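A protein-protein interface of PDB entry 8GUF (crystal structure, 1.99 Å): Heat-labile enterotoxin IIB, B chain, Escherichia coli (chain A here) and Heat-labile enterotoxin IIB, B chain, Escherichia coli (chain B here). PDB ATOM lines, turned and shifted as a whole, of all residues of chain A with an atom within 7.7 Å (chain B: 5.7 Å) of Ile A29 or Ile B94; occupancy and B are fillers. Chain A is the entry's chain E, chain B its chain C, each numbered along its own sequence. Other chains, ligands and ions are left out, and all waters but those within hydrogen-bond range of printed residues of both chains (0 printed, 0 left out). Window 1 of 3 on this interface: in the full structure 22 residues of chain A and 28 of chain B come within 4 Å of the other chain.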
ATOM      1  N   LYS A  27      -7.867  -5.164  -2.295  1.00  0.00           N
ATOM      2  CA  LYS A  27      -9.191  -5.015  -2.850  1.00  0.00           C
ATOM      3  C   LYS A  27      -9.637  -3.570  -2.681  1.00  0.00           C
ATOM      4  O   LYS A  27      -9.366  -2.953  -1.658  1.00  0.00           O
ATOM      5  CB  LYS A  27     -10.245  -5.840  -2.120  1.00  0.00           C
ATOM      6  CG  LYS A  27      -9.856  -7.260  -1.738  1.00  0.00           C
ATOM      7  CD  LYS A  27     -10.094  -8.297  -2.768  1.00  0.00           C
ATOM      8  CE  LYS A  27      -9.868  -9.680  -2.167  1.00  0.00           C
ATOM      9  NZ  LYS A  27     -10.710 -10.673  -2.847  1.00  0.00           N
ATOM     10  N   TYR A  28     -10.304  -3.075  -3.708  1.00  0.00           N
ATOM     11  CA  TYR A  28     -10.877  -1.736  -3.702  1.00  0.00           C
ATOM     12  C   TYR A  28     -12.346  -1.882  -4.090  1.00  0.00           C
ATOM     13  O   TYR A  28     -12.633  -2.449  -5.145  1.00  0.00           O
ATOM     14  CB  TYR A  28     -10.102  -0.873  -4.700  1.00  0.00           C
ATOM     15  CG  TYR A  28     -10.514   0.580  -4.806  1.00  0.00           C
ATOM     16  CD1 TYR A  28     -10.396   1.428  -3.714  1.00  0.00           C
ATOM     17  CD2 TYR A  28     -10.934   1.131  -6.012  1.00  0.00           C
ATOM     18  CE1 TYR A  28     -10.704   2.779  -3.809  1.00  0.00           C
ATOM     19  CE2 TYR A  28     -11.266   2.477  -6.117  1.00  0.00           C
ATOM     20  CZ  TYR A  28     -11.119   3.310  -5.016  1.00  0.00           C
ATOM     21  OH  TYR A  28     -11.437   4.648  -5.035  1.00  0.00           O
ATOM     22  N   ILE A  29     -13.247  -1.349  -3.252  1.00  0.00           N
ATOM     23  CA  ILE A  29     -14.669  -1.591  -3.384  1.00  0.00           C
ATOM     24  C   ILE A  29     -15.424  -0.265  -3.488  1.00  0.00           C
ATOM     25  O   ILE A  29     -15.209   0.624  -2.674  1.00  0.00           O
ATOM     26  CB  ILE A  29     -15.178  -2.396  -2.179  1.00  0.00           C
ATOM     27  CG1 ILE A  29     -14.489  -3.751  -2.089  1.00  0.00           C
ATOM     28  CG2 ILE A  29     -16.699  -2.544  -2.224  1.00  0.00           C
ATOM     29  CD1 ILE A  29     -14.803  -4.485  -0.825  1.00  0.00           C
ATOM     30  N   SER A  30     -16.298  -0.175  -4.490  1.00  0.00           N
ATOM     31  CA  SER A  30     -17.334   0.847  -4.573  1.00  0.00           C
ATOM     32  C   SER A  30     -18.700   0.187  -4.427  1.00  0.00           C
ATOM     33  O   SER A  30     -18.985  -0.772  -5.135  1.00  0.00           O
ATOM     34  CB  SER A  30     -17.285   1.596  -5.875  1.00  0.00           C
ATOM     35  OG  SER A  30     -18.341   2.564  -5.933  1.00  0.00           O
ATOM     36  N   ASP A  31     -19.549   0.758  -3.573  1.00  0.00           N
ATOM     37  CA  ASP A  31     -20.856   0.205  -3.242  1.00  0.00           C
ATOM     38  C   ASP A  31     -21.873   1.346  -3.119  1.00  0.00           C
ATOM     39  O   ASP A  31     -21.631   2.273  -2.346  1.00  0.00           O
ATOM     40  CB  ASP A  31     -20.728  -0.601  -1.938  1.00  0.00           C
ATOM     41  CG  ASP A  31     -21.934  -1.429  -1.488  1.00  0.00           C
ATOM     42  OD1 ASP A  31     -23.081  -1.141  -1.951  1.00  0.00           O
ATOM     43  OD2 ASP A  31     -21.720  -2.375  -0.691  1.00  0.00           O
ATOM     44  N   ILE A  32     -23.021   1.243  -3.828  1.00  0.00           N
ATOM     45  CA  ILE A  32     -24.093   2.226  -3.685  1.00  0.00           C
ATOM     46  C   ILE A  32     -25.367   1.637  -3.073  1.00  0.00           C
ATOM     47  O   ILE A  32     -26.377   2.335  -3.018  1.00  0.00           O
ATOM     48  CB  ILE A  32     -24.420   2.926  -5.017  1.00  0.00           C
ATOM     49  CG1 ILE A  32     -24.763   1.934  -6.130  1.00  0.00           C
ATOM     50  CG2 ILE A  32     -23.298   3.871  -5.403  1.00  0.00           C
ATOM     51  CD1 ILE A  32     -25.509   2.554  -7.275  1.00  0.00           C
ATOM     52  N   ASN A  33     -25.323   0.390  -2.584  1.00  0.00           N
ATOM     53  CA  ASN A  33     -26.456  -0.212  -1.883  1.00  0.00           C
ATOM     54  C   ASN A  33     -26.760   0.600  -0.627  1.00  0.00           C
ATOM     55  O   ASN A  33     -25.850   1.134  -0.012  1.00  0.00           O
ATOM     56  CB  ASN A  33     -26.201  -1.698  -1.610  1.00  0.00           C
ATOM     57  CG  ASN A  33     -26.286  -2.511  -2.889  1.00  0.00           C
ATOM     58  OD1 ASN A  33     -27.250  -2.372  -3.639  1.00  0.00           O
ATOM     59  ND2 ASN A  33     -25.306  -3.370  -3.139  1.00  0.00           N
ATOM     60  N   THR A  36     -24.900  -0.122   2.715  1.00  0.00           N
ATOM     61  CA  THR A  36     -23.460  -0.348   2.767  1.00  0.00           C
ATOM     62  C   THR A  36     -22.749   0.640   1.837  1.00  0.00           C
ATOM     63  O   THR A  36     -21.597   0.452   1.485  1.00  0.00           O
ATOM     64  CB  THR A  36     -23.186  -1.840   2.539  1.00  0.00           C
ATOM     65  OG1 THR A  36     -23.762  -2.228   1.288  1.00  0.00           O
ATOM     66  CG2 THR A  36     -23.765  -2.695   3.647  1.00  0.00           C
ATOM     67  N   GLY A  38     -20.675   3.254   0.155  1.00  0.00           N
ATOM     68  CA  GLY A  38     -19.371   3.781   0.524  1.00  0.00           C
ATOM     69  C   GLY A  38     -18.224   3.243  -0.333  1.00  0.00           C
ATOM     70  O   GLY A  38     -18.419   2.424  -1.211  1.00  0.00           O
ATOM     71  N   MET A  39     -17.032   3.745  -0.037  1.00  0.00           N
ATOM     72  CA  MET A  39     -15.789   3.285  -0.626  1.00  0.00           C
ATOM     73  C   MET A  39     -15.011   2.553   0.457  1.00  0.00           C
ATOM     74  O   MET A  39     -14.837   3.104   1.543  1.00  0.00           O
ATOM     75  CB  MET A  39     -14.968   4.493  -1.099  1.00  0.00           C
ATOM     76  CG  MET A  39     -15.566   5.229  -2.298  1.00  0.00           C
ATOM     77  SD  MET A  39     -15.920   4.161  -3.701  1.00  0.00           S
ATOM     78  CE  MET A  39     -14.340   3.301  -3.838  1.00  0.00           C
ATOM     79  N   TYR A  40     -14.504   1.354   0.132  1.00  0.00           N
ATOM     80  CA  TYR A  40     -13.757   0.544   1.079  1.00  0.00           C
ATOM     81  C   TYR A  40     -12.515  -0.079   0.446  1.00  0.00           C
ATOM     82  O   TYR A  40     -12.422  -0.238  -0.767  1.00  0.00           O
ATOM     83  CB  TYR A  40     -14.606  -0.626   1.590  1.00  0.00           C
ATOM     84  CG  TYR A  40     -15.989  -0.274   2.072  1.00  0.00           C
ATOM     85  CD1 TYR A  40     -17.057  -0.250   1.197  1.00  0.00           C
ATOM     86  CD2 TYR A  40     -16.229   0.045   3.394  1.00  0.00           C
ATOM     87  CE1 TYR A  40     -18.332   0.112   1.617  1.00  0.00           C
ATOM     88  CE2 TYR A  40     -17.502   0.391   3.841  1.00  0.00           C
ATOM     89  CZ  TYR A  40     -18.558   0.411   2.946  1.00  0.00           C
ATOM     90  OH  TYR A  40     -19.821   0.732   3.345  1.00  0.00           O
ATOM     91  N   VAL A  41     -11.608  -0.530   1.314  1.00  0.00           N
ATOM     92  CA  VAL A  41     -10.438  -1.291   0.918  1.00  0.00           C
ATOM     93  C   VAL A  41     -10.297  -2.485   1.845  1.00  0.00           C
ATOM     94  O   VAL A  41     -10.711  -2.414   3.003  1.00  0.00           O
ATOM     95  CB  VAL A  41      -9.157  -0.439   0.989  1.00  0.00           C
ATOM     96  CG1 VAL A  41      -9.091   0.576  -0.141  1.00  0.00           C
ATOM     97  CG2 VAL A  41      -8.999   0.259   2.333  1.00  0.00           C
ATOM     98  N   VAL A  42      -9.603  -3.513   1.334  1.00  0.00           N
ATOM     99  CA  VAL A  42      -9.335  -4.738   2.073  1.00  0.00           C
ATOM    100  C   VAL A  42      -7.848  -5.070   1.916  1.00  0.00           C
ATOM    101  O   VAL A  42      -7.277  -4.893   0.842  1.00  0.00           O
ATOM    102  CB  VAL A  42     -10.237  -5.902   1.603  1.00  0.00           C
ATOM    103  CG1 VAL A  42     -10.059  -7.133   2.495  1.00  0.00           C
ATOM    104  CG2 VAL A  42     -11.709  -5.477   1.511  1.00  0.00           C
ATOM    105  N   VAL A  48     -10.510  -4.566   6.932  1.00  0.00           N
ATOM    106  CA  VAL A  48     -11.441  -3.809   6.098  1.00  0.00           C
ATOM    107  C   VAL A  48     -11.487  -2.366   6.616  1.00  0.00           C
ATOM    108  O   VAL A  48     -11.478  -2.159   7.826  1.00  0.00           O
ATOM    109  CB  VAL A  48     -12.839  -4.450   6.070  1.00  0.00           C
ATOM    110  CG1 VAL A  48     -13.813  -3.638   5.222  1.00  0.00           C
ATOM    111  CG2 VAL A  48     -12.808  -5.902   5.594  1.00  0.00           C
ATOM    112  N   TRP A  49     -11.416  -1.369   5.707  1.00  0.00           N
ATOM    113  CA  TRP A  49     -11.564   0.034   6.098  1.00  0.00           C
ATOM    114  C   TRP A  49     -12.516   0.750   5.151  1.00  0.00           C
ATOM    115  O   TRP A  49     -12.574   0.445   3.964  1.00  0.00           O
ATOM    116  CB  TRP A  49     -10.241   0.813   6.121  1.00  0.00           C
ATOM    117  CG  TRP A  49      -9.256   0.364   7.145  1.00  0.00           C
ATOM    118  CD1 TRP A  49      -8.986   0.944   8.351  1.00  0.00           C
ATOM    119  CD2 TRP A  49      -8.365  -0.749   7.026  1.00  0.00           C
ATOM    120  NE1 TRP A  49      -7.989   0.264   8.987  1.00  0.00           N
ATOM    121  CE2 TRP A  49      -7.605  -0.793   8.210  1.00  0.00           C
ATOM    122  CE3 TRP A  49      -8.147  -1.714   6.044  1.00  0.00           C
ATOM    123  CZ2 TRP A  49      -6.637  -1.768   8.441  1.00  0.00           C
ATOM    124  CZ3 TRP A  49      -7.210  -2.688   6.283  1.00  0.00           C
ATOM    125  CH2 TRP A  49      -6.457  -2.706   7.458  1.00  0.00           C
ATOM    126  N   ILE A  51     -13.232   4.489   3.446  1.00  0.00           N
ATOM    127  CA  ILE A  51     -12.510   5.714   3.118  1.00  0.00           C
ATOM    128  C   ILE A  51     -13.403   6.903   3.488  1.00  0.00           C
ATOM    129  O   ILE A  51     -14.602   6.855   3.242  1.00  0.00           O
ATOM    130  CB  ILE A  51     -12.128   5.722   1.625  1.00  0.00           C
ATOM    131  CG1 ILE A  51     -11.310   4.486   1.230  1.00  0.00           C
ATOM    132  CG2 ILE A  51     -11.418   7.013   1.272  1.00  0.00           C
ATOM    133  CD1 ILE A  51     -10.965   4.437  -0.243  1.00  0.00           C
ATOM    134  N   ALA A  70      -5.638   4.906  -2.442  1.00  0.00           N
ATOM    135  CA  ALA A  70      -6.140   3.544  -2.284  1.00  0.00           C
ATOM    136  C   ALA A  70      -6.030   2.760  -3.580  1.00  0.00           C
ATOM    137  O   ALA A  70      -5.571   1.612  -3.566  1.00  0.00           O
ATOM    138  CB  ALA A  70      -7.574   3.537  -1.835  1.00  0.00           C
ATOM    139  N   VAL A  74      -3.584  -0.496  -4.708  1.00  0.00           N
ATOM    140  CA  VAL A  74      -4.183  -1.748  -5.159  1.00  0.00           C
ATOM    141  C   VAL A  74      -3.552  -2.181  -6.485  1.00  0.00           C
ATOM    142  O   VAL A  74      -3.136  -3.334  -6.605  1.00  0.00           O
ATOM    143  CB  VAL A  74      -5.727  -1.703  -5.237  1.00  0.00           C
ATOM    144  CG1 VAL A  74      -6.278  -2.961  -5.901  1.00  0.00           C
ATOM    145  CG2 VAL A  74      -6.380  -1.549  -3.875  1.00  0.00           C
ATOM    146  N   SER B   3     -14.056 -10.840  -1.273  1.00  0.00           N
ATOM    147  CA  SER B   3     -13.904 -10.802   0.174  1.00  0.00           C
ATOM    148  C   SER B   3     -15.223 -11.158   0.856  1.00  0.00           C
ATOM    149  O   SER B   3     -16.299 -11.009   0.281  1.00  0.00           O
ATOM    150  CB  SER B   3     -13.466  -9.451   0.636  1.00  0.00           C
ATOM    151  OG  SER B   3     -14.515  -8.533   0.365  1.00  0.00           O
ATOM    152  N   PHE B   5     -16.475  -9.613   3.306  1.00  0.00           N
ATOM    153  CA  PHE B   5     -17.101  -8.314   3.491  1.00  0.00           C
ATOM    154  C   PHE B   5     -18.003  -7.981   2.306  1.00  0.00           C
ATOM    155  O   PHE B   5     -19.158  -7.562   2.470  1.00  0.00           O
ATOM    156  CB  PHE B   5     -16.021  -7.248   3.716  1.00  0.00           C
ATOM    157  CG  PHE B   5     -16.572  -5.855   3.834  1.00  0.00           C
ATOM    158  CD1 PHE B   5     -17.105  -5.407   5.029  1.00  0.00           C
ATOM    159  CD2 PHE B   5     -16.591  -5.012   2.732  1.00  0.00           C
ATOM    160  CE1 PHE B   5     -17.633  -4.127   5.126  1.00  0.00           C
ATOM    161  CE2 PHE B   5     -17.141  -3.743   2.825  1.00  0.00           C
ATOM    162  CZ  PHE B   5     -17.660  -3.301   4.020  1.00  0.00           C
ATOM    163  N   PHE B   6     -17.450  -8.147   1.101  1.00  0.00           N
ATOM    164  CA  PHE B   6     -18.186  -7.869  -0.128  1.00  0.00           C
ATOM    165  C   PHE B   6     -19.399  -8.793  -0.282  1.00  0.00           C
ATOM    166  O   PHE B   6     -20.482  -8.332  -0.665  1.00  0.00           O
ATOM    167  CB  PHE B   6     -17.264  -8.017  -1.337  1.00  0.00           C
ATOM    168  CG  PHE B   6     -17.856  -7.446  -2.604  1.00  0.00           C
ATOM    169  CD1 PHE B   6     -17.941  -6.071  -2.801  1.00  0.00           C
ATOM    170  CD2 PHE B   6     -18.380  -8.280  -3.568  1.00  0.00           C
ATOM    171  CE1 PHE B   6     -18.479  -5.551  -3.960  1.00  0.00           C
ATOM    172  CE2 PHE B   6     -18.927  -7.758  -4.730  1.00  0.00           C
ATOM    173  CZ  PHE B   6     -18.984  -6.396  -4.919  1.00  0.00           C
ATOM    174  N   LEU B  23     -13.043  -8.457 -17.352  1.00  0.00           N
ATOM    175  CA  LEU B  23     -13.639  -7.454 -18.220  1.00  0.00           C
ATOM    176  C   LEU B  23     -12.696  -7.174 -19.378  1.00  0.00           C
ATOM    177  O   LEU B  23     -11.555  -6.794 -19.145  1.00  0.00           O
ATOM    178  CB  LEU B  23     -13.909  -6.173 -17.415  1.00  0.00           C
ATOM    179  CG  LEU B  23     -14.900  -6.318 -16.266  1.00  0.00           C
ATOM    180  CD1 LEU B  23     -15.107  -4.980 -15.546  1.00  0.00           C
ATOM    181  CD2 LEU B  23     -16.213  -6.876 -16.784  1.00  0.00           C
ATOM    182  N   GLU B  63     -15.986   6.130  -9.047  1.00  0.00           N
ATOM    183  CA  GLU B  63     -15.005   5.090  -8.736  1.00  0.00           C
ATOM    184  C   GLU B  63     -15.326   3.770  -9.437  1.00  0.00           C
ATOM    185  O   GLU B  63     -14.398   3.036  -9.817  1.00  0.00           O
ATOM    186  CB  GLU B  63     -14.889   4.892  -7.223  1.00  0.00           C
ATOM    187  CG  GLU B  63     -14.374   6.117  -6.459  1.00  0.00           C
ATOM    188  CD  GLU B  63     -13.092   6.725  -7.001  1.00  0.00           C
ATOM    189  OE1 GLU B  63     -12.146   5.954  -7.206  1.00  0.00           O
ATOM    190  OE2 GLU B  63     -13.042   7.966  -7.214  1.00  0.00           O
ATOM    191  N   MET B  64     -16.618   3.460  -9.663  1.00  0.00           N
ATOM    192  CA  MET B  64     -16.965   2.246 -10.405  1.00  0.00           C
ATOM    193  C   MET B  64     -16.424   2.337 -11.825  1.00  0.00           C
ATOM    194  O   MET B  64     -15.900   1.353 -12.363  1.00  0.00           O
ATOM    195  CB  MET B  64     -18.479   2.023 -10.502  1.00  0.00           C
ATOM    196  CG  MET B  64     -19.108   1.583  -9.239  1.00  0.00           C
ATOM    197  SD  MET B  64     -20.910   1.508  -9.449  1.00  0.00           S
ATOM    198  CE  MET B  64     -21.396   0.878  -7.847  1.00  0.00           C
ATOM    199  N   ILE B  67     -12.625   1.779 -11.668  1.00  0.00           N
ATOM    200  CA  ILE B  67     -12.415   0.350 -11.467  1.00  0.00           C
ATOM    201  C   ILE B  67     -12.608  -0.407 -12.776  1.00  0.00           C
ATOM    202  O   ILE B  67     -11.792  -1.276 -13.106  1.00  0.00           O
ATOM    203  CB  ILE B  67     -13.364  -0.178 -10.366  1.00  0.00           C
ATOM    204  CG1 ILE B  67     -12.913   0.287  -8.984  1.00  0.00           C
ATOM    205  CG2 ILE B  67     -13.511  -1.700 -10.426  1.00  0.00           C
ATOM    206  CD1 ILE B  67     -13.931   0.042  -7.895  1.00  0.00           C
ATOM    207  N   ALA B  68     -13.682  -0.064 -13.509  1.00  0.00           N
ATOM    208  CA  ALA B  68     -14.002  -0.704 -14.776  1.00  0.00           C
ATOM    209  C   ALA B  68     -12.854  -0.507 -15.766  1.00  0.00           C
ATOM    210  O   ALA B  68     -12.365  -1.468 -16.348  1.00  0.00           O
ATOM    211  CB  ALA B  68     -15.312  -0.173 -15.333  1.00  0.00           C
ATOM    212  N   VAL B  78     -12.505  -8.596 -11.308  1.00  0.00           N
ATOM    213  CA  VAL B  78     -13.474  -7.922 -10.459  1.00  0.00           C
ATOM    214  C   VAL B  78     -14.483  -8.933  -9.908  1.00  0.00           C
ATOM    215  O   VAL B  78     -14.712  -9.969 -10.516  1.00  0.00           O
ATOM    216  CB  VAL B  78     -14.175  -6.781 -11.223  1.00  0.00           C
ATOM    217  CG1 VAL B  78     -13.157  -5.804 -11.785  1.00  0.00           C
ATOM    218  CG2 VAL B  78     -15.096  -7.290 -12.327  1.00  0.00           C
ATOM    219  N   ASN B  79     -15.033  -8.619  -8.732  1.00  0.00           N
ATOM    220  CA  ASN B  79     -16.254  -9.224  -8.218  1.00  0.00           C
ATOM    221  C   ASN B  79     -17.344  -8.170  -8.253  1.00  0.00           C
ATOM    222  O   ASN B  79     -17.058  -6.993  -8.015  1.00  0.00           O
ATOM    223  CB  ASN B  79     -16.044  -9.737  -6.801  1.00  0.00           C
ATOM    224  CG  ASN B  79     -14.775 -10.551  -6.698  1.00  0.00           C
ATOM    225  OD1 ASN B  79     -13.905 -10.249  -5.885  1.00  0.00           O
ATOM    226  ND2 ASN B  79     -14.661 -11.572  -7.519  1.00  0.00           N
ATOM    227  N   MET B  80     -18.574  -8.594  -8.558  1.00  0.00           N
ATOM    228  CA  MET B  80     -19.648  -7.654  -8.803  1.00  0.00           C
ATOM    229  C   MET B  80     -20.918  -8.090  -8.096  1.00  0.00           C
ATOM    230  O   MET B  80     -21.223  -9.272  -8.035  1.00  0.00           O
ATOM    231  CB  MET B  80     -19.965  -7.578 -10.296  1.00  0.00           C
ATOM    232  CG  MET B  80     -18.920  -6.803 -11.091  1.00  0.00           C
ATOM    233  SD  MET B  80     -19.471  -6.540 -12.793  1.00  0.00           S
ATOM    234  CE  MET B  80     -19.876  -8.227 -13.240  1.00  0.00           C
ATOM    235  N   CYS B  81     -21.662  -7.094  -7.621  1.00  0.00           N
ATOM    236  CA  CYS B  81     -22.997  -7.260  -7.073  1.00  0.00           C
ATOM    237  C   CYS B  81     -23.952  -6.607  -8.068  1.00  0.00           C
ATOM    238  O   CYS B  81     -23.947  -5.386  -8.198  1.00  0.00           O
ATOM    239  CB  CYS B  81     -23.065  -6.612  -5.688  1.00  0.00           C
ATOM    240  SG  CYS B  81     -24.628  -6.872  -4.810  1.00  0.00           S
ATOM    241  N   ILE B  91     -24.703  -2.770 -12.172  1.00  0.00           N
ATOM    242  CA  ILE B  91     -23.739  -2.939 -11.091  1.00  0.00           C
ATOM    243  C   ILE B  91     -24.055  -1.992  -9.932  1.00  0.00           C
ATOM    244  O   ILE B  91     -24.033  -0.775 -10.121  1.00  0.00           O
ATOM    245  CB  ILE B  91     -22.307  -2.697 -11.602  1.00  0.00           C
ATOM    246  CG1 ILE B  91     -21.892  -3.756 -12.622  1.00  0.00           C
ATOM    247  CG2 ILE B  91     -21.341  -2.619 -10.431  1.00  0.00           C
ATOM    248  CD1 ILE B  91     -20.730  -3.340 -13.498  1.00  0.00           C
ATOM    249  N   TRP B  92     -24.321  -2.578  -8.753  1.00  0.00           N
ATOM    250  CA  TRP B  92     -24.623  -1.851  -7.530  1.00  0.00           C
ATOM    251  C   TRP B  92     -23.408  -1.823  -6.595  1.00  0.00           C
ATOM    252  O   TRP B  92     -23.309  -0.941  -5.741  1.00  0.00           O
ATOM    253  CB  TRP B  92     -25.847  -2.451  -6.815  1.00  0.00           C
ATOM    254  CG  TRP B  92     -27.170  -2.165  -7.470  1.00  0.00           C
ATOM    255  CD1 TRP B  92     -27.415  -1.323  -8.521  1.00  0.00           C
ATOM    256  CD2 TRP B  92     -28.436  -2.761  -7.137  1.00  0.00           C
ATOM    257  NE1 TRP B  92     -28.747  -1.326  -8.845  1.00  0.00           N
ATOM    258  CE2 TRP B  92     -29.398  -2.206  -8.017  1.00  0.00           C
ATOM    259  CE3 TRP B  92     -28.854  -3.668  -6.154  1.00  0.00           C
ATOM    260  CZ2 TRP B  92     -30.752  -2.540  -7.945  1.00  0.00           C
ATOM    261  CZ3 TRP B  92     -30.186  -4.011  -6.093  1.00  0.00           C
ATOM    262  CH2 TRP B  92     -31.116  -3.465  -6.986  1.00  0.00           C
ATOM    263  N   ALA B  93     -22.481  -2.776  -6.767  1.00  0.00           N
ATOM    264  CA  ALA B  93     -21.202  -2.725  -6.064  1.00  0.00           C
ATOM    265  C   ALA B  93     -20.137  -3.467  -6.865  1.00  0.00           C
ATOM    266  O   ALA B  93     -20.439  -4.420  -7.575  1.00  0.00           O
ATOM    267  CB  ALA B  93     -21.332  -3.319  -4.661  1.00  0.00           C
ATOM    268  N   ILE B  94     -18.871  -3.066  -6.717  1.00  0.00           N
ATOM    269  CA  ILE B  94     -17.828  -3.741  -7.467  1.00  0.00           C
ATOM    270  C   ILE B  94     -16.543  -3.736  -6.648  1.00  0.00           C
ATOM    271  O   ILE B  94     -16.296  -2.797  -5.908  1.00  0.00           O
ATOM    272  CB  ILE B  94     -17.714  -3.109  -8.872  1.00  0.00           C
ATOM    273  CG1 ILE B  94     -16.677  -3.811  -9.748  1.00  0.00           C
ATOM    274  CG2 ILE B  94     -17.460  -1.604  -8.787  1.00  0.00           C
ATOM    275  CD1 ILE B  94     -16.775  -3.478 -11.212  1.00  0.00           C
ATOM    276  N   GLU B  95     -15.806  -4.856  -6.729  1.00  0.00           N
ATOM    277  CA  GLU B  95     -14.575  -5.090  -5.993  1.00  0.00           C
ATOM    278  C   GLU B  95     -13.451  -5.366  -6.986  1.00  0.00           C
ATOM    279  O   GLU B  95     -13.523  -6.344  -7.738  1.00  0.00           O
ATOM    280  CB  GLU B  95     -14.779  -6.264  -5.025  1.00  0.00           C
ATOM    281  CG  GLU B  95     -13.559  -6.640  -4.202  1.00  0.00           C
ATOM    282  CD  GLU B  95     -13.885  -7.667  -3.128  1.00  0.00           C
ATOM    283  OE1 GLU B  95     -14.154  -8.826  -3.481  1.00  0.00           O
ATOM    284  OE2 GLU B  95     -13.923  -7.293  -1.939  1.00  0.00           O
ATOM    285  N   LEU B  96     -12.436  -4.491  -6.969  1.00  0.00           N
ATOM    286  CA  LEU B  96     -11.230  -4.618  -7.780  1.00  0.00           C
ATOM    287  C   LEU B  96     -10.189  -5.454  -7.034  1.00  0.00           C
ATOM    288  O   LEU B  96      -9.808  -5.133  -5.902  1.00  0.00           O
ATOM    289  CB  LEU B  96     -10.666  -3.230  -8.112  1.00  0.00           C
ATOM    290  CG  LEU B  96      -9.451  -3.208  -9.048  1.00  0.00           C
ATOM    291  CD1 LEU B  96      -9.783  -3.762 -10.436  1.00  0.00           C
ATOM    292  CD2 LEU B  96      -8.882  -1.808  -9.170  1.00  0.00           C
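Printed residues of chain B within 4 Å of Ile A29: Phe B6 (3.8 Å), Ile B94 (3.2 Å) and Glu B95 (3.1 Å).
Of chain A, only Tyr A28 (3.8 Å), Ile A29 (3.2 Å) and Ser A30 (2.8 Å) come within 4 Å of Ile B94.
Of the printed residues of chain A, Ala B93 touches Ser A30 and Asp A31.
Printed residues of chain B within 4 Å of Ser A30: Met B64 (3.5 Å), Ala B93 (3.1 Å) and Ile B94 (2.8 Å).
Printed residues of chain B within 4 Å of Asp A31: Trp B92 (3.7 Å) and Ala B93 (3.7 Å).
The nearest residue of chain A that does not touch Ile B94 is Asp A31 (5.0 Å).
O of Trp B92 is in hydrogen-bond range of N of Ile A32.
O of Ser A30 sits at hydrogen-bond distance from N of Ile B94, 2.8 Å away.
The side-chain amino group (NZ) of Lys A27 is in salt-bridge range of the side-chain carboxylate (OE1) of Glu B95 (3.96 Å).
The backbone carbonyl oxygen of Tyr A28 sits at hydrogen-bond distance from the backbone NH of Leu B96.
OE1 of Glu B63 sits at hydrogen-bond distance from OH of Tyr A28 (2.6 Å).
Printed residues of chain B that touch a printed residue of chain A: Ser B3, Phe B5, Phe B6, Glu B63, Met B64, Ile B67, Cys B81, Trp B92, Ala B93, Ile B94, Glu B95 and Leu B96.
Hydrophobic or aromatic side chains of chain B that line the printed part of chain A: Phe B5, Phe B6, Met B64, Ile B67, Trp B92, Ala B93 and Leu B96.
Hydrophobic or aromatic side chains of chain A that line the printed part of chain B: Tyr A28, Ile A29, Ile A32, Met A39, Tyr A40 and Val A48.
Along chain A the printed residues that touch a printed residue of chain B span positions 27 to 48.
Among the printed residues, 23 pairs touch across the chains.
Among the printed residues, merely in contact across the chains: Lys A27 with Ser B3 (3.7 Å), Lys A27 with Leu B96 (3.1 Å), Tyr A28 with Ile B67 (3.7 Å), Tyr A28 with Ile B94 (3.8 Å), Tyr A28 with Glu B95 (3.4 Å), Ile A29 with Phe B6 (3.8 Å), Ile A29 with Ile B94 (3.2 Å), Ile A29 with Glu B95 (3.1 Å), Ser A30 with Met B64 (3.5 Å), Ser A30 with Ala B93 (3.1 Å), Asp A31 with Trp B92 (3.7 Å), Asp A31 with Ala B93 (3.7 Å), Ile A32 with Met B64 (3.9 Å), Asn A33 with Cys B81 (3.9 Å), Asn A33 with Trp B92 (3.3 Å), Met A39 with Glu B63 (3.7 Å), Tyr A40 with Phe B5 (3.7 Å) and Val A48 with Phe B5 (3.7 Å).
The backbone carbonyl oxygen (O) of Asp A31 is in hydrogen-bond range of the backbone NH (N) of Gly A38 (2.9 Å).
The backbone NH of Asn A33 is in hydrogen-bond range of the side-chain carboxylate of Asp A31, at 2.8 Å.
The backbone NH of Ile A29 lies within hydrogen-bond range of the backbone carbonyl oxygen of Tyr A40.
The backbone NH (N) of Phe B6 sits at hydrogen-bond distance from the side-chain hydroxyl (OG) of Ser B3 (3.1 Å).
N of Glu B95 sits at hydrogen-bond distance from O of Asn B79, at 2.8 Å.
The backbone NH (N) of Cys B81 sits at hydrogen-bond distance from the backbone carbonyl oxygen (O) of Ala B93 (2.9 Å).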
